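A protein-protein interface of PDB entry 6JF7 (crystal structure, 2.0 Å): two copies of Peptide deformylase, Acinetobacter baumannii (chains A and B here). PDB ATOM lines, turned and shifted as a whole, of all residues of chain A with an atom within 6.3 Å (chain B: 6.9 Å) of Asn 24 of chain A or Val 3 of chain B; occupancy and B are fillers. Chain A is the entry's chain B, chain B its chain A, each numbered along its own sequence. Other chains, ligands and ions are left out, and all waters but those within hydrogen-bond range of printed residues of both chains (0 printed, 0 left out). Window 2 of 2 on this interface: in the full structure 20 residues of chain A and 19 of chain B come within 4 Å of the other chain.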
ATOM      1  N   SER A  22       8.326  32.182  18.122  1.00  0.00           N
ATOM      2  CA  SER A  22       9.141  31.123  18.666  1.00  0.00           C
ATOM      3  C   SER A  22      10.566  31.333  18.165  1.00  0.00           C
ATOM      4  O   SER A  22      10.858  32.115  17.249  1.00  0.00           O
ATOM      5  CB  SER A  22       8.637  29.777  18.222  1.00  0.00           C
ATOM      6  OG  SER A  22       8.622  29.710  16.783  1.00  0.00           O
ATOM      7  N   ALA A  23      11.428  30.584  18.779  1.00  0.00           N
ATOM      8  CA  ALA A  23      12.854  30.634  18.516  1.00  0.00           C
ATOM      9  C   ALA A  23      13.238  30.332  17.056  1.00  0.00           C
ATOM     10  O   ALA A  23      14.023  31.078  16.416  1.00  0.00           O
ATOM     11  CB  ALA A  23      13.558  29.704  19.519  1.00  0.00           C
ATOM     12  N   ASN A  24      12.648  29.272  16.503  1.00  0.00           N
ATOM     13  CA  ASN A  24      12.902  28.924  15.110  1.00  0.00           C
ATOM     14  C   ASN A  24      12.525  29.996  14.067  1.00  0.00           C
ATOM     15  O   ASN A  24      13.010  30.007  12.930  1.00  0.00           O
ATOM     16  CB  ASN A  24      12.237  27.596  14.796  1.00  0.00           C
ATOM     17  CG  ASN A  24      12.587  27.087  13.437  1.00  0.00           C
ATOM     18  OD1 ASN A  24      13.775  26.889  13.071  1.00  0.00           O
ATOM     19  ND2 ASN A  24      11.569  26.842  12.672  1.00  0.00           N
ATOM     20  N   GLU A  25      11.626  30.894  14.439  1.00  0.00           N
ATOM     21  CA  GLU A  25      11.156  31.976  13.560  1.00  0.00           C
ATOM     22  C   GLU A  25      12.093  33.181  13.584  1.00  0.00           C
ATOM     23  O   GLU A  25      12.056  33.943  12.659  1.00  0.00           O
ATOM     24  CB  GLU A  25       9.745  32.461  13.961  1.00  0.00           C
ATOM     25  CG  GLU A  25       8.597  31.509  13.744  1.00  0.00           C
ATOM     26  CD  GLU A  25       7.286  32.027  14.419  1.00  0.00           C
ATOM     27  OE1 GLU A  25       6.984  31.629  15.563  1.00  0.00           O
ATOM     28  OE2 GLU A  25       6.604  32.900  13.800  1.00  0.00           O
ATOM     29  N   LEU A  26      12.939  33.337  14.593  1.00  0.00           N
ATOM     30  CA  LEU A  26      13.877  34.434  14.632  1.00  0.00           C
ATOM     31  C   LEU A  26      14.874  34.304  13.493  1.00  0.00           C
ATOM     32  O   LEU A  26      15.276  33.195  13.162  1.00  0.00           O
ATOM     33  CB  LEU A  26      14.614  34.466  15.972  1.00  0.00           C
ATOM     34  CG  LEU A  26      13.688  34.622  17.159  1.00  0.00           C
ATOM     35  CD1 LEU A  26      14.405  34.349  18.478  1.00  0.00           C
ATOM     36  CD2 LEU A  26      13.108  36.035  17.118  1.00  0.00           C
ATOM     37  N   ASN A  27      15.173  35.438  12.848  1.00  0.00           N
ATOM     38  CA  ASN A  27      16.129  35.530  11.751  1.00  0.00           C
ATOM     39  C   ASN A  27      15.677  34.679  10.548  1.00  0.00           C
ATOM     40  O   ASN A  27      16.505  34.128   9.818  1.00  0.00           O
ATOM     41  CB  ASN A  27      17.529  35.098  12.270  1.00  0.00           C
ATOM     42  CG  ASN A  27      18.678  35.596  11.396  1.00  0.00           C
ATOM     43  OD1 ASN A  27      19.742  34.947  11.341  1.00  0.00           O
ATOM     44  ND2 ASN A  27      18.487  36.712  10.722  1.00  0.00           N
ATOM     45  N   SER A  28      14.364  34.530  10.369  1.00  0.00           N
ATOM     46  CA  SER A  28      13.837  33.761   9.236  1.00  0.00           C
ATOM     47  C   SER A  28      13.250  34.688   8.178  1.00  0.00           C
ATOM     48  O   SER A  28      12.843  35.802   8.503  1.00  0.00           O
ATOM     49  CB  SER A  28      12.796  32.760   9.700  1.00  0.00           C
ATOM     50  OG  SER A  28      11.514  33.364   9.959  1.00  0.00           O
ATOM     51  N   VAL B   2      11.305  26.956   8.117  1.00  0.00           N
ATOM     52  CA  VAL B   2      10.689  27.322   9.403  1.00  0.00           C
ATOM     53  C   VAL B   2       9.486  26.475   9.725  1.00  0.00           C
ATOM     54  O   VAL B   2       8.529  26.361   8.963  1.00  0.00           O
ATOM     55  CB  VAL B   2      10.231  28.788   9.440  1.00  0.00           C
ATOM     56  CG1 VAL B   2       9.480  29.123  10.728  1.00  0.00           C
ATOM     57  CG2 VAL B   2      11.431  29.670   9.371  1.00  0.00           C
ATOM     58  N   VAL B   3       9.508  25.933  10.910  1.00  0.00           N
ATOM     59  CA  VAL B   3       8.429  25.111  11.409  1.00  0.00           C
ATOM     60  C   VAL B   3       7.743  26.088  12.342  1.00  0.00           C
ATOM     61  O   VAL B   3       8.379  26.619  13.264  1.00  0.00           O
ATOM     62  CB  VAL B   3       8.991  23.864  12.114  1.00  0.00           C
ATOM     63  CG1 VAL B   3       7.948  23.135  12.950  1.00  0.00           C
ATOM     64  CG2 VAL B   3       9.593  22.935  11.056  1.00  0.00           C
ATOM     65  N   LEU B   4       6.459  26.293  12.117  1.00  0.00           N
ATOM     66  CA  LEU B   4       5.671  27.217  12.943  1.00  0.00           C
ATOM     67  C   LEU B   4       5.011  26.557  14.136  1.00  0.00           C
ATOM     68  O   LEU B   4       4.667  25.429  14.054  1.00  0.00           O
ATOM     69  CB  LEU B   4       4.624  27.893  12.080  1.00  0.00           C
ATOM     70  CG  LEU B   4       5.112  28.797  10.975  1.00  0.00           C
ATOM     71  CD1 LEU B   4       3.947  29.230  10.097  1.00  0.00           C
ATOM     72  CD2 LEU B   4       5.756  30.015  11.638  1.00  0.00           C
ATOM     73  N   PRO B   5       4.870  27.260  15.265  1.00  0.00           N
ATOM     74  CA  PRO B   5       4.142  26.640  16.394  1.00  0.00           C
ATOM     75  C   PRO B   5       2.625  26.508  16.083  1.00  0.00           C
ATOM     76  O   PRO B   5       2.050  27.301  15.326  1.00  0.00           O
ATOM     77  CB  PRO B   5       4.379  27.598  17.543  1.00  0.00           C
ATOM     78  CG  PRO B   5       4.761  28.917  16.928  1.00  0.00           C
ATOM     79  CD  PRO B   5       5.445  28.567  15.624  1.00  0.00           C
ATOM     80  N   ALA B  37       6.164  27.883   4.884  1.00  0.00           N
ATOM     81  CA  ALA B  37       6.157  27.633   6.311  1.00  0.00           C
ATOM     82  C   ALA B  37       5.014  26.724   6.768  1.00  0.00           C
ATOM     83  O   ALA B  37       5.234  25.844   7.603  1.00  0.00           O
ATOM     84  CB  ALA B  37       6.136  28.933   7.113  1.00  0.00           C
ATOM     85  N   ALA B  40       6.085  23.138   5.474  1.00  0.00           N
ATOM     86  CA  ALA B  40       7.099  22.588   6.364  1.00  0.00           C
ATOM     87  C   ALA B  40       6.543  22.184   7.733  1.00  0.00           C
ATOM     88  O   ALA B  40       6.932  21.150   8.288  1.00  0.00           O
ATOM     89  CB  ALA B  40       8.251  23.576   6.540  1.00  0.00           C
ATOM     90  N   THR B  41       5.660  22.988   8.314  1.00  0.00           N
ATOM     91  CA  THR B  41       5.067  22.622   9.576  1.00  0.00           C
ATOM     92  C   THR B  41       4.268  21.326   9.456  1.00  0.00           C
ATOM     93  O   THR B  41       4.381  20.478  10.316  1.00  0.00           O
ATOM     94  CB  THR B  41       4.216  23.782  10.083  1.00  0.00           C
ATOM     95  OG1 THR B  41       5.038  24.959  10.151  1.00  0.00           O
ATOM     96  CG2 THR B  41       3.581  23.472  11.441  1.00  0.00           C
ATOM     97  N   MET B  42       3.451  21.205   8.409  1.00  0.00           N
ATOM     98  CA  MET B  42       2.605  20.020   8.166  1.00  0.00           C
ATOM     99  C   MET B  42       3.463  18.759   8.071  1.00  0.00           C
ATOM    100  O   MET B  42       3.208  17.768   8.763  1.00  0.00           O
ATOM    101  CB  MET B  42       1.829  20.215   6.851  1.00  0.00           C
ATOM    102  CG  MET B  42       0.846  19.106   6.485  1.00  0.00           C
ATOM    103  SD  MET B  42       0.318  19.277   4.776  1.00  0.00           S
ATOM    104  CE  MET B  42       1.839  18.992   3.840  1.00  0.00           C
ATOM    105  N   GLU B  44       6.634  18.302   9.335  1.00  0.00           N
ATOM    106  CA  GLU B  44       7.315  18.007  10.584  1.00  0.00           C
ATOM    107  C   GLU B  44       6.379  17.350  11.609  1.00  0.00           C
ATOM    108  O   GLU B  44       6.818  16.590  12.454  1.00  0.00           O
ATOM    109  CB  GLU B  44       7.900  19.309  11.178  1.00  0.00           C
ATOM    110  CG  GLU B  44       8.533  19.223  12.585  1.00  0.00           C
ATOM    111  CD  GLU B  44       9.980  18.710  12.625  1.00  0.00           C
ATOM    112  OE1 GLU B  44      10.697  18.800  11.591  1.00  0.00           O
ATOM    113  OE2 GLU B  44      10.418  18.242  13.717  1.00  0.00           O
ATOM    114  N   ARG B  45       5.099  17.682  11.553  1.00  0.00           N
ATOM    115  CA  ARG B  45       4.083  17.088  12.406  1.00  0.00           C
ATOM    116  C   ARG B  45       3.389  15.866  11.799  1.00  0.00           C
ATOM    117  O   ARG B  45       2.419  15.400  12.363  1.00  0.00           O
ATOM    118  CB  ARG B  45       3.045  18.154  12.755  1.00  0.00           C
ATOM    119  CG  ARG B  45       3.624  19.383  13.443  1.00  0.00           C
ATOM    120  CD  ARG B  45       3.982  19.136  14.913  1.00  0.00           C
ATOM    121  NE  ARG B  45       4.300  20.417  15.566  1.00  0.00           N
ATOM    122  CZ  ARG B  45       3.665  20.996  16.604  1.00  0.00           C
ATOM    123  NH1 ARG B  45       4.094  22.200  17.045  1.00  0.00           N
ATOM    124  NH2 ARG B  45       2.635  20.420  17.241  1.00  0.00           N
ATOM    125  N   VAL B  55      -1.615  27.844  12.587  1.00  0.00           N
ATOM    126  CA  VAL B  55      -0.305  28.425  12.860  1.00  0.00           C
ATOM    127  C   VAL B  55      -0.398  29.923  13.248  1.00  0.00           C
ATOM    128  O   VAL B  55       0.508  30.705  12.986  1.00  0.00           O
ATOM    129  CB  VAL B  55       0.714  28.138  11.721  1.00  0.00           C
ATOM    130  CG1 VAL B  55       1.025  26.654  11.699  1.00  0.00           C
ATOM    131  CG2 VAL B  55       0.187  28.627  10.385  1.00  0.00           C
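The backbone NH of Val 3 of chain B sits close to the side-chain amide nitrogen of Asn 24 of chain A.
No position is printed for both chains.
Of the 7 printed residues of chain A, 4 touch a printed residue of chain B.
Hydrophobic or aromatic side chains of chain B within 4 Å of the printed part of chain A: Val 2, Val 3, Leu 4 and Pro 5.
Among the printed residues, 7 pairs touch across the chains.
Among the printed residues, no Asp or Glu carboxylate lies within 4 Å of a Lys or Arg side-chain nitrogen of the other chain.
Printed residues of chain B within 4 Å of Ser 22 of chain A: Pro 5.
Asn 24 of chain A touches just these residues of chain B: Val 2 (3.4 Å) and Val 3 (2.9 Å).
Of the printed residues of chain B, Glu 25 of chain A touches Val 2 (3.9 Å), Leu 4 (3.7 Å) and Pro 5 (3.4 Å).
Printed residues of chain A within 4 Å of Val 2 of chain B: Asn 24 (3.4 Å), Glu 25 (3.9 Å) and Ser 28 (3.4 Å).
Of chain A, only Asn 24 comes within 4 Å of Val 3 of chain B.
Printed residues of chain A within 4 Å of Leu 4 of chain B: Glu 25 (3.7 Å).
Of the printed residues of chain A, Pro 5 of chain B touches Ser 22 and Glu 25.
The nearest residue of chain B that does not touch Asn 24 of chain A is Leu 4 of chain B (5.2 Å).
The nearest residue of chain A that does not touch Val 3 of chain B is Ser 22 of chain A (4.7 Å).
The nearest printed residue of chain B that does not touch Ser 28 of chain A is Leu 4 of chain B (6.9 Å).
Among the printed residues, merely in contact across the chains: Ser 22 of chain A with Pro 5 of chain B, Asn 24 of chain A with Val 2 of chain B, Glu 25 of chain A with Val 2 of chain B, Glu 25 of chain A with Leu 4 of chain B, Glu 25 of chain A with Pro 5 of chain B and Ser 28 of chain A with Val 2 of chain B.
OG of Ser 28 of chain A sits at hydrogen-bond distance from O of Glu 25 of chain A (2.8 Å).
The side-chain carboxylate (OE1) of Glu 25 of chain A lies within hydrogen-bond range of the side-chain hydroxyl (OG) of Ser 22 of chain A (2.8 Å).
The side-chain hydroxyl (OG1) of Thr 41 of chain B sits at hydrogen-bond distance from the backbone NH (N) of Leu 4 of chain B (2.8 Å).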
